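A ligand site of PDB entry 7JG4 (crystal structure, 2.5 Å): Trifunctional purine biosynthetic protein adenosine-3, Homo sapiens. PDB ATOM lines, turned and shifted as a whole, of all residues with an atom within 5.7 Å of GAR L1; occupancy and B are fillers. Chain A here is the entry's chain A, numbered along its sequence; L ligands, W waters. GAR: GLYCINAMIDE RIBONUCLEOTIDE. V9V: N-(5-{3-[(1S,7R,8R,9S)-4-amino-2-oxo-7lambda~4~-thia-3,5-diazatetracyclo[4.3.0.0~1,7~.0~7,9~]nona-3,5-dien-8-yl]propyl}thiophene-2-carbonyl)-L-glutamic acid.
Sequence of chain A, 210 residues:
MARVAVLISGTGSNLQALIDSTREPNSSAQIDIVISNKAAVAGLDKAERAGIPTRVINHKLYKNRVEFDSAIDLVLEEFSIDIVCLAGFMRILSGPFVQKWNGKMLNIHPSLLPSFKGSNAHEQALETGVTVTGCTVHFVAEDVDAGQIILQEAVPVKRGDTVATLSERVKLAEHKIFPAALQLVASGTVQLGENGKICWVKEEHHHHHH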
ATOM      1  N   GLY A  10     -16.783  -7.685  -8.979  1.00  0.00           N
ATOM      2  CA  GLY A  10     -17.978  -7.045  -8.484  1.00  0.00           C
ATOM      3  C   GLY A  10     -18.131  -6.899  -6.972  1.00  0.00           C
ATOM      4  O   GLY A  10     -17.275  -6.292  -6.315  1.00  0.00           O
ATOM      5  N   THR A  11     -19.210  -7.457  -6.422  1.00  0.00           N
ATOM      6  CA  THR A  11     -19.621  -7.099  -5.062  1.00  0.00           C
ATOM      7  C   THR A  11     -18.650  -7.604  -4.013  1.00  0.00           C
ATOM      8  O   THR A  11     -18.425  -6.930  -2.991  1.00  0.00           O
ATOM      9  CB  THR A  11     -21.016  -7.650  -4.797  1.00  0.00           C
ATOM     10  OG1 THR A  11     -21.933  -7.093  -5.752  1.00  0.00           O
ATOM     11  CG2 THR A  11     -21.478  -7.301  -3.382  1.00  0.00           C
ATOM     12  N   GLY A  12     -18.095  -8.794  -4.205  1.00  0.00           N
ATOM     13  CA  GLY A  12     -17.072  -9.307  -3.309  1.00  0.00           C
ATOM     14  C   GLY A  12     -17.571 -10.048  -2.096  1.00  0.00           C
ATOM     15  O   GLY A  12     -16.849 -10.111  -1.092  1.00  0.00           O
ATOM     16  N   SER A  13     -18.796 -10.619  -2.132  1.00  0.00           N
ATOM     17  CA  SER A  13     -19.274 -11.366  -0.974  1.00  0.00           C
ATOM     18  C   SER A  13     -18.489 -12.661  -0.778  1.00  0.00           C
ATOM     19  O   SER A  13     -18.279 -13.081   0.365  1.00  0.00           O
ATOM     20  CB  SER A  13     -20.783 -11.655  -1.086  1.00  0.00           C
ATOM     21  OG  SER A  13     -21.121 -12.485  -2.191  1.00  0.00           O
ATOM     22  N   ASN A  14     -18.038 -13.307  -1.863  1.00  0.00           N
ATOM     23  CA  ASN A  14     -17.156 -14.444  -1.666  1.00  0.00           C
ATOM     24  C   ASN A  14     -15.802 -14.000  -1.145  1.00  0.00           C
ATOM     25  O   ASN A  14     -15.233 -14.649  -0.259  1.00  0.00           O
ATOM     26  CB  ASN A  14     -16.993 -15.233  -2.955  1.00  0.00           C
ATOM     27  CG  ASN A  14     -18.192 -16.073  -3.254  1.00  0.00           C
ATOM     28  OD1 ASN A  14     -18.384 -17.138  -2.667  1.00  0.00           O
ATOM     29  ND2 ASN A  14     -19.039 -15.581  -4.158  1.00  0.00           N
ATOM     30  N   LEU A  15     -15.273 -12.890  -1.683  1.00  0.00           N
ATOM     31  CA  LEU A  15     -14.063 -12.304  -1.106  1.00  0.00           C
ATOM     32  C   LEU A  15     -14.233 -12.111   0.386  1.00  0.00           C
ATOM     33  O   LEU A  15     -13.365 -12.502   1.181  1.00  0.00           O
ATOM     34  CB  LEU A  15     -13.733 -10.967  -1.758  1.00  0.00           C
ATOM     35  CG  LEU A  15     -12.581 -10.226  -1.062  1.00  0.00           C
ATOM     36  CD1 LEU A  15     -11.318 -11.047  -1.195  1.00  0.00           C
ATOM     37  CD2 LEU A  15     -12.360  -8.817  -1.617  1.00  0.00           C
ATOM     38  N   ALA A  87     -12.967 -15.157  -7.457  1.00  0.00           N
ATOM     39  CA  ALA A  87     -14.177 -14.957  -6.650  1.00  0.00           C
ATOM     40  C   ALA A  87     -15.051 -13.899  -7.353  1.00  0.00           C
ATOM     41  O   ALA A  87     -15.018 -12.717  -7.012  1.00  0.00           O
ATOM     42  CB  ALA A  87     -13.805 -14.533  -5.215  1.00  0.00           C
ATOM     43  N   GLY A  88     -15.824 -14.348  -8.331  1.00  0.00           N
ATOM     44  CA  GLY A  88     -16.634 -13.416  -9.108  1.00  0.00           C
ATOM     45  C   GLY A  88     -15.863 -12.718 -10.192  1.00  0.00           C
ATOM     46  O   GLY A  88     -16.292 -11.674 -10.683  1.00  0.00           O
ATOM     47  N   PHE A  89     -14.707 -13.268 -10.544  1.00  0.00           N
ATOM     48  CA  PHE A  89     -13.886 -12.729 -11.615  1.00  0.00           C
ATOM     49  C   PHE A  89     -14.472 -13.207 -12.941  1.00  0.00           C
ATOM     50  O   PHE A  89     -14.630 -14.418 -13.148  1.00  0.00           O
ATOM     51  CB  PHE A  89     -12.448 -13.204 -11.427  1.00  0.00           C
ATOM     52  CG  PHE A  89     -11.498 -12.622 -12.395  1.00  0.00           C
ATOM     53  CD1 PHE A  89     -11.023 -11.327 -12.216  1.00  0.00           C
ATOM     54  CD2 PHE A  89     -11.062 -13.358 -13.475  1.00  0.00           C
ATOM     55  CE1 PHE A  89     -10.118 -10.780 -13.114  1.00  0.00           C
ATOM     56  CE2 PHE A  89     -10.161 -12.819 -14.379  1.00  0.00           C
ATOM     57  CZ  PHE A  89      -9.689 -11.528 -14.192  1.00  0.00           C
ATOM     58  N   MET A  90     -14.811 -12.276 -13.814  1.00  0.00           N
ATOM     59  CA  MET A  90     -15.636 -12.594 -14.973  1.00  0.00           C
ATOM     60  C   MET A  90     -14.868 -12.507 -16.287  1.00  0.00           C
ATOM     61  O   MET A  90     -15.452 -12.278 -17.354  1.00  0.00           O
ATOM     62  CB  MET A  90     -16.872 -11.692 -15.030  1.00  0.00           C
ATOM     63  CG  MET A  90     -17.819 -11.880 -13.840  1.00  0.00           C
ATOM     64  SD  MET A  90     -18.330 -13.602 -13.523  1.00  0.00           S
ATOM     65  CE  MET A  90     -18.949 -14.107 -15.144  1.00  0.00           C
ATOM     66  N   ASN A 107     -11.728 -21.678  -8.610  1.00  0.00           N
ATOM     67  CA  ASN A 107     -12.835 -20.875  -9.085  1.00  0.00           C
ATOM     68  C   ASN A 107     -14.123 -21.352  -8.434  1.00  0.00           C
ATOM     69  O   ASN A 107     -14.306 -22.547  -8.217  1.00  0.00           O
ATOM     70  CB  ASN A 107     -12.981 -20.957 -10.602  1.00  0.00           C
ATOM     71  CG  ASN A 107     -14.183 -20.212 -11.108  1.00  0.00           C
ATOM     72  OD1 ASN A 107     -14.273 -18.993 -10.962  1.00  0.00           O
ATOM     73  ND2 ASN A 107     -15.139 -20.930 -11.690  1.00  0.00           N
ATOM     74  N   ILE A 108     -14.998 -20.398  -8.100  1.00  0.00           N
ATOM     75  CA  ILE A 108     -16.334 -20.671  -7.573  1.00  0.00           C
ATOM     76  C   ILE A 108     -17.339 -20.406  -8.686  1.00  0.00           C
ATOM     77  O   ILE A 108     -17.333 -19.330  -9.300  1.00  0.00           O
ATOM     78  CB  ILE A 108     -16.652 -19.852  -6.298  1.00  0.00           C
ATOM     79  CG1 ILE A 108     -18.037 -20.169  -5.758  1.00  0.00           C
ATOM     80  CG2 ILE A 108     -16.587 -18.358  -6.558  1.00  0.00           C
ATOM     81  CD1 ILE A 108     -18.203 -21.516  -5.140  1.00  0.00           C
ATOM     82  N   HIS A 109     -18.185 -21.396  -8.962  1.00  0.00           N
ATOM     83  CA  HIS A 109     -19.200 -21.336 -10.007  1.00  0.00           C
ATOM     84  C   HIS A 109     -20.540 -21.706  -9.385  1.00  0.00           C
ATOM     85  O   HIS A 109     -20.617 -22.710  -8.642  1.00  0.00           O
ATOM     86  CB  HIS A 109     -18.868 -22.275 -11.166  1.00  0.00           C
ATOM     87  CG  HIS A 109     -19.871 -22.284 -12.281  1.00  0.00           C
ATOM     88  ND1 HIS A 109     -19.890 -21.319 -13.271  1.00  0.00           N
ATOM     89  CD2 HIS A 109     -20.874 -23.147 -12.579  1.00  0.00           C
ATOM     90  CE1 HIS A 109     -20.863 -21.595 -14.118  1.00  0.00           C
ATOM     91  NE2 HIS A 109     -21.470 -22.695 -13.728  1.00  0.00           N
ATOM     92  N   PRO A 110     -21.625 -20.942  -9.682  1.00  0.00           N
ATOM     93  CA  PRO A 110     -22.921 -21.132  -9.025  1.00  0.00           C
ATOM     94  C   PRO A 110     -23.802 -22.148  -9.735  1.00  0.00           C
ATOM     95  O   PRO A 110     -24.964 -21.882 -10.061  1.00  0.00           O
ATOM     96  CB  PRO A 110     -23.538 -19.728  -9.085  1.00  0.00           C
ATOM     97  CG  PRO A 110     -23.066 -19.207 -10.461  1.00  0.00           C
ATOM     98  CD  PRO A 110     -21.685 -19.906 -10.729  1.00  0.00           C
ATOM     99  N   GLY A 118     -20.792 -21.675 -17.824  1.00  0.00           N
ATOM    100  CA  GLY A 118     -20.921 -20.351 -18.368  1.00  0.00           C
ATOM    101  C   GLY A 118     -21.465 -19.337 -17.377  1.00  0.00           C
ATOM    102  O   GLY A 118     -21.609 -19.575 -16.176  1.00  0.00           O
ATOM    103  N   SER A 119     -21.785 -18.176 -17.923  1.00  0.00           N
ATOM    104  CA  SER A 119     -21.904 -16.961 -17.115  1.00  0.00           C
ATOM    105  C   SER A 119     -23.285 -16.733 -16.519  1.00  0.00           C
ATOM    106  O   SER A 119     -23.437 -15.825 -15.687  1.00  0.00           O
ATOM    107  CB  SER A 119     -21.510 -15.756 -17.971  1.00  0.00           C
ATOM    108  OG  SER A 119     -22.086 -15.877 -19.255  1.00  0.00           O
ATOM    109  N   HIS A 122     -27.644 -19.495 -13.128  1.00  0.00           N
ATOM    110  CA  HIS A 122     -28.978 -19.379 -12.546  1.00  0.00           C
ATOM    111  C   HIS A 122     -30.077 -19.265 -13.604  1.00  0.00           C
ATOM    112  O   HIS A 122     -31.142 -19.897 -13.465  1.00  0.00           O
ATOM    113  CB  HIS A 122     -29.010 -18.169 -11.620  1.00  0.00           C
ATOM    114  CG  HIS A 122     -28.113 -18.310 -10.443  1.00  0.00           C
ATOM    115  ND1 HIS A 122     -28.118 -19.437  -9.643  1.00  0.00           N
ATOM    116  CD2 HIS A 122     -27.182 -17.489  -9.916  1.00  0.00           C
ATOM    117  CE1 HIS A 122     -27.240 -19.291  -8.680  1.00  0.00           C
ATOM    118  NE2 HIS A 122     -26.649 -18.119  -8.812  1.00  0.00           N
ATOM    119  N   ASP A 145     -14.873 -24.243 -16.516  1.00  0.00           N
ATOM    120  CA  ASP A 145     -15.781 -24.970 -15.620  1.00  0.00           C
ATOM    121  C   ASP A 145     -15.729 -26.478 -15.885  1.00  0.00           C
ATOM    122  O   ASP A 145     -16.743 -27.180 -15.834  1.00  0.00           O
ATOM    123  CB  ASP A 145     -17.207 -24.436 -15.718  1.00  0.00           C
ATOM    124  CG  ASP A 145     -17.268 -22.917 -15.653  1.00  0.00           C
ATOM    125  OD1 ASP A 145     -16.383 -22.303 -15.002  1.00  0.00           O
ATOM    126  OD2 ASP A 145     -18.198 -22.331 -16.259  1.00  0.00           O
ATOM    127  N   LYS A 171     -25.508 -18.203  -2.861  1.00  0.00           N
ATOM    128  CA  LYS A 171     -24.336 -17.523  -2.302  1.00  0.00           C
ATOM    129  C   LYS A 171     -24.104 -17.909  -0.851  1.00  0.00           C
ATOM    130  O   LYS A 171     -22.976 -17.815  -0.378  1.00  0.00           O
ATOM    131  CB  LYS A 171     -24.481 -15.999  -2.428  1.00  0.00           C
ATOM    132  CG  LYS A 171     -24.040 -15.466  -3.787  1.00  0.00           C
ATOM    133  CD  LYS A 171     -23.977 -13.956  -3.789  1.00  0.00           C
ATOM    134  CE  LYS A 171     -23.720 -13.415  -5.189  1.00  0.00           C
ATOM    135  NZ  LYS A 171     -23.569 -11.928  -5.170  1.00  0.00           N
ATOM    136  N   GLU A 174     -22.013 -20.893  -1.341  1.00  0.00           N
ATOM    137  CA  GLU A 174     -20.715 -20.444  -1.839  1.00  0.00           C
ATOM    138  C   GLU A 174     -19.810 -19.985  -0.699  1.00  0.00           C
ATOM    139  O   GLU A 174     -18.645 -20.389  -0.625  1.00  0.00           O
ATOM    140  CB  GLU A 174     -20.934 -19.313  -2.828  1.00  0.00           C
ATOM    141  CG  GLU A 174     -21.725 -19.706  -4.061  1.00  0.00           C
ATOM    142  CD  GLU A 174     -21.738 -18.592  -5.078  1.00  0.00           C
ATOM    143  OE1 GLU A 174     -22.641 -18.533  -5.952  1.00  0.00           O
ATOM    144  OE2 GLU A 174     -20.819 -17.738  -5.004  1.00  0.00           O
ATOM    145  N   HIS A 175     -20.332 -19.144   0.182  1.00  0.00           N
ATOM    146  CA  HIS A 175     -19.574 -18.619   1.308  1.00  0.00           C
ATOM    147  C   HIS A 175     -19.158 -19.679   2.312  1.00  0.00           C
ATOM    148  O   HIS A 175     -18.383 -19.374   3.237  1.00  0.00           O
ATOM    149  CB  HIS A 175     -20.387 -17.537   1.997  1.00  0.00           C
ATOM    150  CG  HIS A 175     -20.824 -16.441   1.077  1.00  0.00           C
ATOM    151  ND1 HIS A 175     -21.904 -15.636   1.347  1.00  0.00           N
ATOM    152  CD2 HIS A 175     -20.326 -16.034  -0.109  1.00  0.00           C
ATOM    153  CE1 HIS A 175     -22.053 -14.759   0.366  1.00  0.00           C
ATOM    154  NE2 HIS A 175     -21.111 -14.977  -0.527  1.00  0.00           N
HETATM  155  C1  GAR L   1     -20.921 -15.541  -7.410  1.00  0.00           C
HETATM  156  O6  GAR L   1     -22.273 -15.889  -7.210  1.00  0.00           O
HETATM  157  C2  GAR L   1     -20.239 -16.572  -8.327  1.00  0.00           C
HETATM  158  O8  GAR L   1     -20.787 -17.867  -8.280  1.00  0.00           O
HETATM  159  C3  GAR L   1     -20.393 -15.932  -9.720  1.00  0.00           C
HETATM  160  O4  GAR L   1     -20.362 -14.506  -9.458  1.00  0.00           O
HETATM  161  C5  GAR L   1     -20.835 -14.191  -8.131  1.00  0.00           C
HETATM  162  C10 GAR L   1     -19.907 -13.209  -7.452  1.00  0.00           C
HETATM  163  O12 GAR L   1     -20.449 -12.754  -6.208  1.00  0.00           O
HETATM  164  N19 GAR L   1     -19.389 -16.351 -10.656  1.00  0.00           N
HETATM  165  C21 GAR L   1     -19.746 -16.901 -11.828  1.00  0.00           C
HETATM  166  O22 GAR L   1     -20.909 -16.934 -12.259  1.00  0.00           O
HETATM  167  C23 GAR L   1     -18.608 -17.488 -12.624  1.00  0.00           C
HETATM  168  N24 GAR L   1     -19.061 -18.056 -13.881  1.00  0.00           N
HETATM  169  P15 GAR L   1     -19.505 -11.913  -5.210  1.00  0.00           P
HETATM  170  O16 GAR L   1     -18.553 -12.934  -4.612  1.00  0.00           O
HETATM  171  O17 GAR L   1     -20.468 -11.295  -4.231  1.00  0.00           O
HETATM  172  O18 GAR L   1     -18.822 -10.900  -6.113  1.00  0.00           O
HETATM  173  C8  V9V L   2     -12.292 -20.307 -15.842  1.00  0.00           C
HETATM  174  C6  V9V L   2     -13.136 -18.523 -14.751  1.00  0.00           C
HETATM  175  N1  V9V L   2     -10.653 -19.507 -17.426  1.00  0.00           N
HETATM  176  C2  V9V L   2     -10.469 -20.824 -17.767  1.00  0.00           C
HETATM  177  N3  V9V L   2     -11.084 -21.890 -17.261  1.00  0.00           N
HETATM  178  C4  V9V L   2     -12.001 -21.666 -16.303  1.00  0.00           C
HETATM  179  C7  V9V L   2     -13.241 -19.840 -14.826  1.00  0.00           C
HETATM  180  C13 V9V L   2     -17.336 -16.844 -18.547  1.00  0.00           C
HETATM  181  C14 V9V L   2     -17.645 -18.083 -18.069  1.00  0.00           C
HETATM  182  C15 V9V L   2     -17.244 -18.237 -16.766  1.00  0.00           C
HETATM  183  C16 V9V L   2     -16.641 -17.156 -16.212  1.00  0.00           C
HETATM  184  C17 V9V L   2     -17.563 -16.219 -19.849  1.00  0.00           C
HETATM  185  C20 V9V L   2     -17.038 -14.026 -21.040  1.00  0.00           C
HETATM  186  C21 V9V L   2     -17.794 -12.775 -20.567  1.00  0.00           C
HETATM  187  C22 V9V L   2     -16.833 -11.634 -20.184  1.00  0.00           C
HETATM  188  C23 V9V L   2     -17.341 -10.693 -19.115  1.00  0.00           C
HETATM  189  C26 V9V L   2     -15.613 -13.664 -21.433  1.00  0.00           C
HETATM  190  C29 V9V L   2     -13.960 -17.676 -13.848  1.00  0.00           C
HETATM  191  C30 V9V L   2     -15.364 -18.143 -14.244  1.00  0.00           C
HETATM  192  C31 V9V L   2     -16.088 -16.954 -14.832  1.00  0.00           C
HETATM  193  C9  V9V L   2     -11.583 -19.255 -16.446  1.00  0.00           C
HETATM  194  N11 V9V L   2      -9.557 -21.063 -18.737  1.00  0.00           N
HETATM  195  N19 V9V L   2     -17.016 -14.979 -19.928  1.00  0.00           N
HETATM  196  O10 V9V L   2     -12.597 -22.610 -15.794  1.00  0.00           O
HETATM  197  O18 V9V L   2     -18.184 -16.780 -20.736  1.00  0.00           O
HETATM  198  O24 V9V L   2     -16.764  -9.651 -18.911  1.00  0.00           O
HETATM  199  O25 V9V L   2     -18.429 -11.009 -18.396  1.00  0.00           O
HETATM  200  O27 V9V L   2     -14.763 -13.413 -20.614  1.00  0.00           O
HETATM  201  O28 V9V L   2     -15.272 -13.617 -22.740  1.00  0.00           O
HETATM  202  S12 V9V L   2     -16.538 -15.885 -17.321  1.00  0.00           S
HETATM  203  S5  V9V L   2     -11.962 -18.056 -15.920  1.00  0.00           S
HETATM  204  O   HOH W   1     -25.375 -17.241  -6.504  1.00  0.00           O
HETATM  205  O   HOH W   2     -22.958 -18.372 -13.924  1.00  0.00           O
HETATM  206  O   HOH W   3     -16.751  -9.996  -7.616  1.00  0.00           O
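An oxygen (O17) of GAR L1 sits at hydrogen-bond distance from the backbone NH (N) of Ser 13. The side-chain hydroxyl (OG) of Ser 13 lies within hydrogen-bond range of an oxygen (O17) of GAR L1 (2.5 Å). An oxygen (O16) of GAR L1 lies within hydrogen-bond range of the backbone NH (N) of Asn 14 (2.8 Å). O16 of GAR L1 sits at hydrogen-bond distance from ND2 of Asn 14. The backbone NH (N) of Gly 12 lies within hydrogen-bond range of an oxygen (O18) of GAR L1 (2.9 Å). OE1 of Glu 174 sits at hydrogen-bond distance from O6 of GAR L1 (3.0 Å). An oxygen (O17) of GAR L1 lies within salt-bridge range of the side-chain amino group of Lys 171, 3.3 Å away. A ring nitrogen (ND1) of His 109 sits at hydrogen-bond distance from a nitrogen (N24) of GAR L1 (3.4 Å). N of Thr 11 lies within hydrogen-bond range of O18 of GAR L1, 3.5 Å away. An oxygen (O10) of V9V L2 lies within hydrogen-bond range of the backbone NH (N) of Asp 145, 2.9 Å away.
A ring nitrogen (NE2) of His 175 lies within hydrogen-bond range of the side-chain hydroxyl (OG) of Ser 13 (3.0 Å). OE2 of Glu 174 lies within hydrogen-bond range of ND2 of Asn 14 (2.9 Å). ND1 of His 175 sits close to O of Lys 171, 3.0 Å away. The side-chain carboxylate (OD2) of Asp 145 sits at hydrogen-bond distance from the backbone NH (N) of Gly 118 (3.1 Å).
The backbone nitrogen (N) of Pro 110 lies close to an oxygen (O8) of GAR L1 (3.5 Å). CA of Gly 88 touches C10 of GAR L1 (3.7 Å). SD of Met 90 touches C21 of GAR L1, 3.97 Å away. Ile 108 touches GAR L1. Gly 118 touches GAR L1 (O to N24, 3.8 Å). Of the 21 residues printed, 12 come within 4 Å of GAR L1. The nearest printed residue that does not touch GAR L1 is Gly 10 (4.2 Å).
Water W3 lies within hydrogen-bond range of the backbone NH of Gly 10, an oxygen (O18) of GAR L1 and the backbone carbonyl oxygen of Ala 87. Water W1 lies within hydrogen-bond range of NE2 of His 122 (2.8 Å), OE1 of Glu 174 (3.1 Å) and O6 of GAR L1 (3.5 Å).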
